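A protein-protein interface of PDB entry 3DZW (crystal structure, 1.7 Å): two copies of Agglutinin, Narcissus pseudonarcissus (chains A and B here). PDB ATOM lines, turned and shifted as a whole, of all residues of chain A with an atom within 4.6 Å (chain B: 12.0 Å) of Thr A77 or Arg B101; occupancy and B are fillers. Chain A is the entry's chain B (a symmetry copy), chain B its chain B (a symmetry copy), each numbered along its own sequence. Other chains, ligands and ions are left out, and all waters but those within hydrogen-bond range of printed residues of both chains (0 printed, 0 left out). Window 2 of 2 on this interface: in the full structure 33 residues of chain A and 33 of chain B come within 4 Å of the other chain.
Thr A77 touches Arg B101, and with the chains exchanged Arg A101 touches Thr B77.
Ile A96 touches Arg B101, and with the chains exchanged Arg A101 touches Ile B96.
Gly A98 touches Arg B101, and with the chains exchanged Arg A101 touches Gly B98.
Thr A99 touches Arg B101, and with the chains exchanged Arg A101 touches Thr B99.
7 positions are printed for both chains.
Of the 16 pairs that touch across the chains among the printed residues, 11 have their exchanged pair printed and touching as well.
Of the 20 printed residues of chain B, 8 touch a printed residue of chain A.
Of the 13 printed residues of chain A, 6 touch a printed residue of chain B.
Among the printed residues, no Asp or Glu carboxylate lies within 4 Å of a Lys or Arg side-chain nitrogen of the other chain.
Printed residues of chain B within 4 Å of Thr A77: Arg B101 (3.7 Å) and Trp B102 (3.6 Å).
Of the printed residues of chain A, Arg B101 touches Thr A77 (3.7 Å), Ile A96 (2.9 Å), Gly A98 (2.9 Å) and Thr A99 (3.9 Å).
No residue of chain B comes within 4 Å of Asp A59.
Gly A60 touches none of the printed residues of chain B.
No residue of chain B comes within 4 Å of Asn A61.
No residue of chain B comes within 4 Å of Leu A62.
Printed residues of chain B within 4 Å of Ser A75: Trp B102.
No residue of chain B comes within 4 Å of Asn A76.
No residue of chain B comes within 4 Å of Gly A78.
No residue of chain B comes within 4 Å of Gly A79.
Printed residues of chain B within 4 Å of Ile A96: Ala B100 (3.5 Å), Arg B101 (2.9 Å) and Trp B102 (3.0 Å).
Printed residues of chain A within 4 Å of Trp B102: Ser A75 (3.9 Å), Thr A77 (3.6 Å) and Ile A96 (3.0 Å).
Printed residues of chain A within 4 Å of Tyr B97: Thr A99.
Printed residues of chain A within 4 Å of Thr B99: Gly A98 (3.5 Å) and Arg A101 (3.9 Å).
Printed residues of chain A within 4 Å of Thr B77: Arg A101.
Gly B79 touches none of the printed residues of chain A.
The nearest printed residue of chain B that does not touch Arg A101 is Arg B101 (4.1 Å).
Among the printed residues, pairs that only touch across the chains: Ile A96 with Ala B100 (3.5 Å), Thr A77 with Trp B102 (3.6 Å), Arg A101 with Thr B77 (3.7 Å), Thr A77 with Arg B101 (3.7 Å), Thr A99 with Tyr B97 (3.8 Å), Ser A75 with Trp B102 (3.9 Å), Arg A101 with Thr B99 (3.9 Å) and Thr A99 with Arg B101 (3.9 Å).
N of Arg B101 sits at hydrogen-bond distance from O of Ile A96 (2.9 Å).
The backbone NH of Ile A96 lies within hydrogen-bond range of the backbone carbonyl oxygen of Trp B102, 3.0 Å away.
The backbone carbonyl oxygen (O) of Thr A99 sits close to the backbone carbonyl oxygen (O) of Gly B98 (3.5 Å).
The guanidinium group (NE) of Arg A101 lies within hydrogen-bond range of the backbone carbonyl oxygen (O) of Gly B98, 2.9 Å away.
The backbone NH (N) of Arg A101 sits at hydrogen-bond distance from the backbone carbonyl oxygen (O) of Ile B96 (2.9 Å).
O of Thr B99 sits close to O of Gly A98 (3.5 Å).
NE of Arg B101 sits at hydrogen-bond distance from O of Gly A98 (2.9 Å).
O of Gly A98 lies close to O of Gly B98, 3.0 Å away.
The backbone carbonyl oxygen of Leu A62 is in hydrogen-bond range of the backbone NH of Ser A75.
O of Gly A60 lies within hydrogen-bond range of OG1 of Thr A77, at 2.6 Å.
OD1 of Asn A61 sits at hydrogen-bond distance from N of Thr A77.
O of Val B85 lies within hydrogen-bond range of N of Tyr B97 (2.9 Å).
O of Gly B60 sits at hydrogen-bond distance from OG1 of Thr B77, at 2.6 Å.
OD1 of Asn A61 lies within hydrogen-bond range of OG of Ser A75 (3.3 Å).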
ATOM      1  N   ASP A  59     -18.281  12.650   0.940  1.00  0.00           N
ATOM      2  CA  ASP A  59     -18.742  14.040   0.780  1.00  0.00           C
ATOM      3  C   ASP A  59     -19.038  14.318  -0.729  1.00  0.00           C
ATOM      4  O   ASP A  59     -19.451  15.412  -1.098  1.00  0.00           O
ATOM      5  CB  ASP A  59     -17.751  15.085   1.389  1.00  0.00           C
ATOM      6  CG  ASP A  59     -16.394  15.168   0.640  1.00  0.00           C
ATOM      7  OD1 ASP A  59     -16.117  14.337  -0.239  1.00  0.00           O
ATOM      8  OD2 ASP A  59     -15.609  16.096   0.960  1.00  0.00           O
ATOM      9  N   GLY A  60     -18.810  13.298  -1.580  1.00  0.00           N
ATOM     10  CA  GLY A  60     -19.074  13.397  -3.021  1.00  0.00           C
ATOM     11  C   GLY A  60     -17.894  13.829  -3.886  1.00  0.00           C
ATOM     12  O   GLY A  60     -18.025  13.916  -5.091  1.00  0.00           O
ATOM     13  N   ASN A  61     -16.737  14.077  -3.267  1.00  0.00           N
ATOM     14  CA  ASN A  61     -15.568  14.520  -3.991  1.00  0.00           C
ATOM     15  C   ASN A  61     -14.669  13.316  -4.395  1.00  0.00           C
ATOM     16  O   ASN A  61     -14.436  12.412  -3.588  1.00  0.00           O
ATOM     17  CB  ASN A  61     -14.792  15.538  -3.126  1.00  0.00           C
ATOM     18  CG  ASN A  61     -13.867  16.491  -3.959  1.00  0.00           C
ATOM     19  OD1 ASN A  61     -13.980  16.594  -5.182  1.00  0.00           O
ATOM     20  ND2 ASN A  61     -12.988  17.217  -3.257  1.00  0.00           N
ATOM     21  N   LEU A  62     -14.213  13.301  -5.658  1.00  0.00           N
ATOM     22  CA  LEU A  62     -13.311  12.258  -6.186  1.00  0.00           C
ATOM     23  C   LEU A  62     -11.934  12.866  -6.136  1.00  0.00           C
ATOM     24  O   LEU A  62     -11.682  13.858  -6.799  1.00  0.00           O
ATOM     25  CB  LEU A  62     -13.704  11.864  -7.609  1.00  0.00           C
ATOM     26  CG  LEU A  62     -12.901  10.755  -8.319  1.00  0.00           C
ATOM     27  CD1 LEU A  62     -13.037   9.405  -7.602  1.00  0.00           C
ATOM     28  CD2 LEU A  62     -13.334  10.622  -9.763  1.00  0.00           C
ATOM     29  N   SER A  75     -12.252  16.431  -8.344  1.00  0.00           N
ATOM     30  CA  SER A  75     -13.377  16.807  -9.201  1.00  0.00           C
ATOM     31  C   SER A  75     -14.091  18.095  -8.712  1.00  0.00           C
ATOM     32  O   SER A  75     -14.872  18.680  -9.453  1.00  0.00           O
ATOM     33  CB  SER A  75     -14.384  15.650  -9.307  1.00  0.00           C
ATOM     34  OG  SER A  75     -14.882  15.276  -8.042  1.00  0.00           O
ATOM     35  N   ASN A  76     -13.804  18.521  -7.465  1.00  0.00           N
ATOM     36  CA  ASN A  76     -14.418  19.729  -6.868  1.00  0.00           C
ATOM     37  C   ASN A  76     -15.936  19.576  -6.693  1.00  0.00           C
ATOM     38  O   ASN A  76     -16.700  20.535  -6.893  1.00  0.00           O
ATOM     39  CB  ASN A  76     -14.088  20.997  -7.694  1.00  0.00           C
ATOM     40  CG  ASN A  76     -12.573  21.272  -7.797  1.00  0.00           C
ATOM     41  OD1 ASN A  76     -11.813  21.017  -6.862  1.00  0.00           O
ATOM     42  ND2 ASN A  76     -12.155  21.822  -8.925  1.00  0.00           N
ATOM     43  N   THR A  77     -16.365  18.368  -6.311  1.00  0.00           N
ATOM     44  CA  THR A  77     -17.788  18.068  -6.117  1.00  0.00           C
ATOM     45  C   THR A  77     -18.122  17.712  -4.655  1.00  0.00           C
ATOM     46  O   THR A  77     -19.072  16.965  -4.386  1.00  0.00           O
ATOM     47  CB  THR A  77     -18.252  16.927  -7.072  1.00  0.00           C
ATOM     48  OG1 THR A  77     -17.428  15.763  -6.880  1.00  0.00           O
ATOM     49  CG2 THR A  77     -18.152  17.372  -8.504  1.00  0.00           C
ATOM     50  N   GLY A  78     -17.342  18.260  -3.714  1.00  0.00           N
ATOM     51  CA  GLY A  78     -17.570  18.023  -2.299  1.00  0.00           C
ATOM     52  C   GLY A  78     -18.837  18.741  -1.866  1.00  0.00           C
ATOM     53  O   GLY A  78     -19.107  19.856  -2.312  1.00  0.00           O
ATOM     54  N   GLY A  79     -19.621  18.101  -1.014  1.00  0.00           N
ATOM     55  CA  GLY A  79     -20.866  18.690  -0.537  1.00  0.00           C
ATOM     56  C   GLY A  79     -21.417  17.957   0.665  1.00  0.00           C
ATOM     57  O   GLY A  79     -20.677  17.646   1.600  1.00  0.00           O
ATOM     58  N   ILE A  96     -19.866  10.941 -11.986  1.00  0.00           N
ATOM     59  CA  ILE A  96     -20.170  10.876 -10.550  1.00  0.00           C
ATOM     60  C   ILE A  96     -21.655  11.186 -10.321  1.00  0.00           C
ATOM     61  O   ILE A  96     -22.134  12.249 -10.745  1.00  0.00           O
ATOM     62  CB  ILE A  96     -19.342  11.873  -9.725  1.00  0.00           C
ATOM     63  CG1 ILE A  96     -17.856  11.562  -9.817  1.00  0.00           C
ATOM     64  CG2 ILE A  96     -19.769  11.833  -8.252  1.00  0.00           C
ATOM     65  CD1 ILE A  96     -16.958  12.595  -9.093  1.00  0.00           C
ATOM     66  N   GLY A  98     -25.013  11.198  -7.375  1.00  0.00           N
ATOM     67  CA  GLY A  98     -25.366  11.209  -5.951  1.00  0.00           C
ATOM     68  C   GLY A  98     -26.147  12.456  -5.571  1.00  0.00           C
ATOM     69  O   GLY A  98     -26.199  13.393  -6.354  1.00  0.00           O
ATOM     70  N   THR A  99     -26.755  12.477  -4.368  1.00  0.00           N
ATOM     71  CA  THR A  99     -26.694  11.357  -3.406  1.00  0.00           C
ATOM     72  C   THR A  99     -27.781  10.290  -3.716  1.00  0.00           C
ATOM     73  O   THR A  99     -28.487  10.391  -4.726  1.00  0.00           O
ATOM     74  CB  THR A  99     -26.839  11.858  -1.953  1.00  0.00           C
ATOM     75  OG1 THR A  99     -26.544  10.793  -1.038  1.00  0.00           O
ATOM     76  CG2 THR A  99     -28.256  12.393  -1.695  1.00  0.00           C
ATOM     77  N   ARG A 101     -31.223   8.597  -3.728  1.00  0.00           N
ATOM     78  CA  ARG A 101     -32.604   9.109  -3.621  1.00  0.00           C
ATOM     79  C   ARG A 101     -33.587   8.080  -3.054  1.00  0.00           C
ATOM     80  O   ARG A 101     -34.559   8.443  -2.375  1.00  0.00           O
ATOM     81  CB  ARG A 101     -33.110   9.559  -4.996  1.00  0.00           C
ATOM     82  CG  ARG A 101     -32.249  10.615  -5.704  1.00  0.00           C
ATOM     83  CD  ARG A 101     -32.145  11.901  -4.909  1.00  0.00           C
ATOM     84  NE  ARG A 101     -31.437  12.948  -5.651  1.00  0.00           N
ATOM     85  CZ  ARG A 101     -31.179  14.169  -5.167  1.00  0.00           C
ATOM     86  NH1 ARG A 101     -31.573  14.512  -3.932  1.00  0.00           N
ATOM     87  NH2 ARG A 101     -30.526  15.057  -5.917  1.00  0.00           N
ATOM     88  N   SER B   6     -31.087   6.587 -16.907  1.00  0.00           N
ATOM     89  CA  SER B   6     -32.276   7.402 -17.141  1.00  0.00           C
ATOM     90  C   SER B   6     -32.450   7.543 -18.643  1.00  0.00           C
ATOM     91  O   SER B   6     -31.475   7.803 -19.374  1.00  0.00           O
ATOM     92  CB  SER B   6     -32.180   8.769 -16.453  1.00  0.00           C
ATOM     93  OG  SER B   6     -31.037   9.482 -16.872  1.00  0.00           O
ATOM     94  N   GLY B  60     -35.920  11.583 -12.547  1.00  0.00           N
ATOM     95  CA  GLY B  60     -35.406  10.834 -11.394  1.00  0.00           C
ATOM     96  C   GLY B  60     -36.356   9.803 -10.793  1.00  0.00           C
ATOM     97  O   GLY B  60     -36.000   9.127  -9.848  1.00  0.00           O
ATOM     98  N   THR B  77     -39.532   9.559  -6.471  1.00  0.00           N
ATOM     99  CA  THR B  77     -38.298  10.352  -6.447  1.00  0.00           C
ATOM    100  C   THR B  77     -38.202  11.331  -7.635  1.00  0.00           C
ATOM    101  O   THR B  77     -37.102  11.684  -8.077  1.00  0.00           O
ATOM    102  CB  THR B  77     -37.043   9.429  -6.404  1.00  0.00           C
ATOM    103  OG1 THR B  77     -37.070   8.514  -7.514  1.00  0.00           O
ATOM    104  CG2 THR B  77     -37.013   8.648  -5.120  1.00  0.00           C
ATOM    105  N   GLY B  79     -38.173  14.774  -9.582  1.00  0.00           N
ATOM    106  CA  GLY B  79     -37.657  16.089  -9.219  1.00  0.00           C
ATOM    107  C   GLY B  79     -37.111  16.835 -10.415  1.00  0.00           C
ATOM    108  O   GLY B  79     -37.748  16.876 -11.469  1.00  0.00           O
ATOM    109  N   GLU B  80     -35.929  17.428 -10.253  1.00  0.00           N
ATOM    110  CA  GLU B  80     -35.298  18.186 -11.332  1.00  0.00           C
ATOM    111  C   GLU B  80     -34.905  17.290 -12.502  1.00  0.00           C
ATOM    112  O   GLU B  80     -34.561  16.111 -12.311  1.00  0.00           O
ATOM    113  CB  GLU B  80     -34.051  18.947 -10.821  1.00  0.00           C
ATOM    114  CG  GLU B  80     -32.905  18.040 -10.271  1.00  0.00           C
ATOM    115  CD  GLU B  80     -31.669  18.836  -9.832  1.00  0.00           C
ATOM    116  OE1 GLU B  80     -30.733  18.220  -9.280  1.00  0.00           O
ATOM    117  OE2 GLU B  80     -31.638  20.069 -10.036  1.00  0.00           O
ATOM    118  N   ASN B  81     -34.963  17.849 -13.711  1.00  0.00           N
ATOM    119  CA  ASN B  81     -34.593  17.128 -14.905  1.00  0.00           C
ATOM    120  C   ASN B  81     -33.084  16.987 -14.947  1.00  0.00           C
ATOM    121  O   ASN B  81     -32.362  17.950 -14.691  1.00  0.00           O
ATOM    122  CB  ASN B  81     -35.129  17.846 -16.160  1.00  0.00           C
ATOM    123  CG  ASN B  81     -34.758  17.122 -17.476  1.00  0.00           C
ATOM    124  OD1 ASN B  81     -35.634  16.718 -18.234  1.00  0.00           O
ATOM    125  ND2 ASN B  81     -33.468  16.946 -17.722  1.00  0.00           N
ATOM    126  N   GLY B  82     -32.601  15.782 -15.249  1.00  0.00           N
ATOM    127  CA  GLY B  82     -31.166  15.543 -15.313  1.00  0.00           C
ATOM    128  C   GLY B  82     -30.817  14.128 -15.731  1.00  0.00           C
ATOM    129  O   GLY B  82     -31.529  13.513 -16.518  1.00  0.00           O
ATOM    130  N   ASN B  83     -29.698  13.628 -15.201  1.00  0.00           N
ATOM    131  CA  ASN B  83     -29.203  12.279 -15.486  1.00  0.00           C
ATOM    132  C   ASN B  83     -29.138  11.474 -14.215  1.00  0.00           C
ATOM    133  O   ASN B  83     -28.544  11.914 -13.228  1.00  0.00           O
ATOM    134  CB  ASN B  83     -27.834  12.358 -16.144  1.00  0.00           C
ATOM    135  CG  ASN B  83     -27.895  12.970 -17.542  1.00  0.00           C
ATOM    136  OD1 ASN B  83     -28.483  12.400 -18.449  1.00  0.00           O
ATOM    137  ND2 ASN B  83     -27.251  14.107 -17.716  1.00  0.00           N
ATOM    138  N   TYR B  84     -29.744  10.279 -14.242  1.00  0.00           N
ATOM    139  CA  TYR B  84     -29.809   9.387 -13.082  1.00  0.00           C
ATOM    140  C   TYR B  84     -29.458   7.949 -13.445  1.00  0.00           C
ATOM    141  O   TYR B  84     -29.407   7.587 -14.630  1.00  0.00           O
ATOM    142  CB  TYR B  84     -31.223   9.394 -12.493  1.00  0.00           C
ATOM    143  CG  TYR B  84     -31.736  10.749 -12.016  1.00  0.00           C
ATOM    144  CD1 TYR B  84     -32.300  11.663 -12.908  1.00  0.00           C
ATOM    145  CD2 TYR B  84     -31.702  11.089 -10.670  1.00  0.00           C
ATOM    146  CE1 TYR B  84     -32.783  12.897 -12.465  1.00  0.00           C
ATOM    147  CE2 TYR B  84     -32.181  12.319 -10.224  1.00  0.00           C
ATOM    148  CZ  TYR B  84     -32.718  13.211 -11.123  1.00  0.00           C
ATOM    149  OH  TYR B  84     -33.199  14.430 -10.666  1.00  0.00           O
ATOM    150  N   VAL B  85     -29.222   7.125 -12.413  1.00  0.00           N
ATOM    151  CA  VAL B  85     -28.936   5.699 -12.592  1.00  0.00           C
ATOM    152  C   VAL B  85     -29.614   4.840 -11.522  1.00  0.00           C
ATOM    153  O   VAL B  85     -29.664   5.225 -10.363  1.00  0.00           O
ATOM    154  CB  VAL B  85     -27.389   5.362 -12.572  1.00  0.00           C
ATOM    155  CG1 VAL B  85     -26.683   5.933 -13.796  1.00  0.00           C
ATOM    156  CG2 VAL B  85     -26.716   5.829 -11.251  1.00  0.00           C
ATOM    157  N   ILE B  96     -31.123   4.181  -6.451  1.00  0.00           N
ATOM    158  CA  ILE B  96     -31.211   5.268  -7.436  1.00  0.00           C
ATOM    159  C   ILE B  96     -30.286   6.420  -7.019  1.00  0.00           C
ATOM    160  O   ILE B  96     -30.412   6.935  -5.898  1.00  0.00           O
ATOM    161  CB  ILE B  96     -32.635   5.828  -7.574  1.00  0.00           C
ATOM    162  CG1 ILE B  96     -33.594   4.766  -8.088  1.00  0.00           C
ATOM    163  CG2 ILE B  96     -32.650   7.021  -8.536  1.00  0.00           C
ATOM    164  CD1 ILE B  96     -35.069   5.236  -8.148  1.00  0.00           C
ATOM    165  N   TYR B  97     -29.357   6.814  -7.913  1.00  0.00           N
ATOM    166  CA  TYR B  97     -28.419   7.925  -7.658  1.00  0.00           C
ATOM    167  C   TYR B  97     -28.592   9.033  -8.682  1.00  0.00           C
ATOM    168  O   TYR B  97     -28.851   8.765  -9.843  1.00  0.00           O
ATOM    169  CB  TYR B  97     -26.953   7.471  -7.737  1.00  0.00           C
ATOM    170  CG  TYR B  97     -26.477   6.438  -6.710  1.00  0.00           C
ATOM    171  CD1 TYR B  97     -26.507   5.075  -6.997  1.00  0.00           C
ATOM    172  CD2 TYR B  97     -25.939   6.839  -5.479  1.00  0.00           C
ATOM    173  CE1 TYR B  97     -26.043   4.126  -6.072  1.00  0.00           C
ATOM    174  CE2 TYR B  97     -25.479   5.911  -4.556  1.00  0.00           C
ATOM    175  CZ  TYR B  97     -25.531   4.549  -4.855  1.00  0.00           C
ATOM    176  OH  TYR B  97     -25.062   3.626  -3.931  1.00  0.00           O
ATOM    177  N   GLY B  98     -28.413  10.283  -8.254  1.00  0.00           N
ATOM    178  CA  GLY B  98     -28.503  11.427  -9.168  1.00  0.00           C
ATOM    179  C   GLY B  98     -28.701  12.735  -8.419  1.00  0.00           C
ATOM    180  O   GLY B  98     -28.999  12.709  -7.234  1.00  0.00           O
ATOM    181  N   THR B  99     -28.542  13.884  -9.105  1.00  0.00           N
ATOM    182  CA  THR B  99     -28.192  13.934 -10.540  1.00  0.00           C
ATOM    183  C   THR B  99     -26.655  13.827 -10.748  1.00  0.00           C
ATOM    184  O   THR B  99     -25.907  13.615  -9.787  1.00  0.00           O
ATOM    185  CB  THR B  99     -28.732  15.218 -11.205  1.00  0.00           C
ATOM    186  OG1 THR B  99     -28.585  15.130 -12.629  1.00  0.00           O
ATOM    187  CG2 THR B  99     -27.996  16.460 -10.678  1.00  0.00           C
ATOM    188  N   ALA B 100     -26.200  13.966 -12.002  1.00  0.00           N
ATOM    189  CA  ALA B 100     -24.755  13.900 -12.324  1.00  0.00           C
ATOM    190  C   ALA B 100     -24.055  15.158 -11.783  1.00  0.00           C
ATOM    191  O   ALA B 100     -24.475  16.289 -12.085  1.00  0.00           O
ATOM    192  CB  ALA B 100     -24.543  13.772 -13.794  1.00  0.00           C
ATOM    193  N   ARG B 101     -22.998  14.955 -10.986  1.00  0.00           N
ATOM    194  CA  ARG B 101     -22.238  16.066 -10.377  1.00  0.00           C
ATOM    195  C   ARG B 101     -21.026  16.496 -11.208  1.00  0.00           C
ATOM    196  O   ARG B 101     -20.645  17.676 -11.205  1.00  0.00           O
ATOM    197  CB  ARG B 101     -21.753  15.671  -8.977  1.00  0.00           C
ATOM    198  CG  ARG B 101     -22.850  15.230  -7.997  1.00  0.00           C
ATOM    199  CD  ARG B 101     -23.866  16.325  -7.741  1.00  0.00           C
ATOM    200  NE  ARG B 101     -24.830  15.946  -6.704  1.00  0.00           N
ATOM    201  CZ  ARG B 101     -25.852  16.716  -6.309  1.00  0.00           C
ATOM    202  NH1 ARG B 101     -26.051  17.922  -6.860  1.00  0.00           N
ATOM    203  NH2 ARG B 101     -26.680  16.285  -5.357  1.00  0.00           N
ATOM    204  N   TRP B 102     -20.422  15.534 -11.910  1.00  0.00           N
ATOM    205  CA  TRP B 102     -19.237  15.778 -12.718  1.00  0.00           C
ATOM    206  C   TRP B 102     -19.058  14.655 -13.702  1.00  0.00           C
ATOM    207  O   TRP B 102     -19.560  13.555 -13.477  1.00  0.00           O
ATOM    208  CB  TRP B 102     -18.012  15.873 -11.794  1.00  0.00           C
ATOM    209  CG  TRP B 102     -16.651  15.883 -12.486  1.00  0.00           C
ATOM    210  CD1 TRP B 102     -15.944  16.970 -12.885  1.00  0.00           C
ATOM    211  CD2 TRP B 102     -15.850  14.734 -12.826  1.00  0.00           C
ATOM    212  NE1 TRP B 102     -14.753  16.577 -13.460  1.00  0.00           N
ATOM    213  CE2 TRP B 102     -14.675  15.211 -13.436  1.00  0.00           C
ATOM    214  CE3 TRP B 102     -16.022  13.348 -12.680  1.00  0.00           C
ATOM    215  CZ2 TRP B 102     -13.662  14.350 -13.904  1.00  0.00           C
ATOM    216  CZ3 TRP B 102     -15.018  12.493 -13.143  1.00  0.00           C
ATOM    217  CH2 TRP B 102     -13.855  13.003 -13.748  1.00  0.00           C
ATOM    218  N   ALA B 103     -18.350  14.930 -14.810  1.00  0.00           N
ATOM    219  CA  ALA B 103     -18.074  13.910 -15.830  1.00  0.00           C
ATOM    220  C   ALA B 103     -16.853  14.265 -16.667  1.00  0.00           C
ATOM    221  O   ALA B 103     -16.511  15.452 -16.819  1.00  0.00           O
ATOM    222  CB  ALA B 103     -19.281  13.714 -16.734  1.00  0.00           C
ATOM    223  N   THR B 104     -16.188  13.235 -17.204  1.00  0.00           N
ATOM    224  CA  THR B 104     -15.015  13.428 -18.070  1.00  0.00           C
ATOM    225  C   THR B 104     -15.408  14.019 -19.440  1.00  0.00           C
ATOM    226  O   THR B 104     -14.581  14.662 -20.112  1.00  0.00           O
ATOM    227  CB  THR B 104     -14.233  12.109 -18.298  1.00  0.00           C
ATOM    228  OG1 THR B 104     -15.132  11.085 -18.775  1.00  0.00           O
ATOM    229  CG2 THR B 104     -13.578  11.643 -17.019  1.00  0.00           C
ATOM    230  N   GLY B 105     -16.666  13.793 -19.845  1.00  0.00           N
ATOM    231  CA  GLY B 105     -17.184  14.292 -21.123  1.00  0.00           C
ATOM    232  C   GLY B 105     -16.635  13.532 -22.313  1.00  0.00           C
ATOM    233  O   GLY B 105     -16.517  14.085 -23.412  1.00  0.00           O
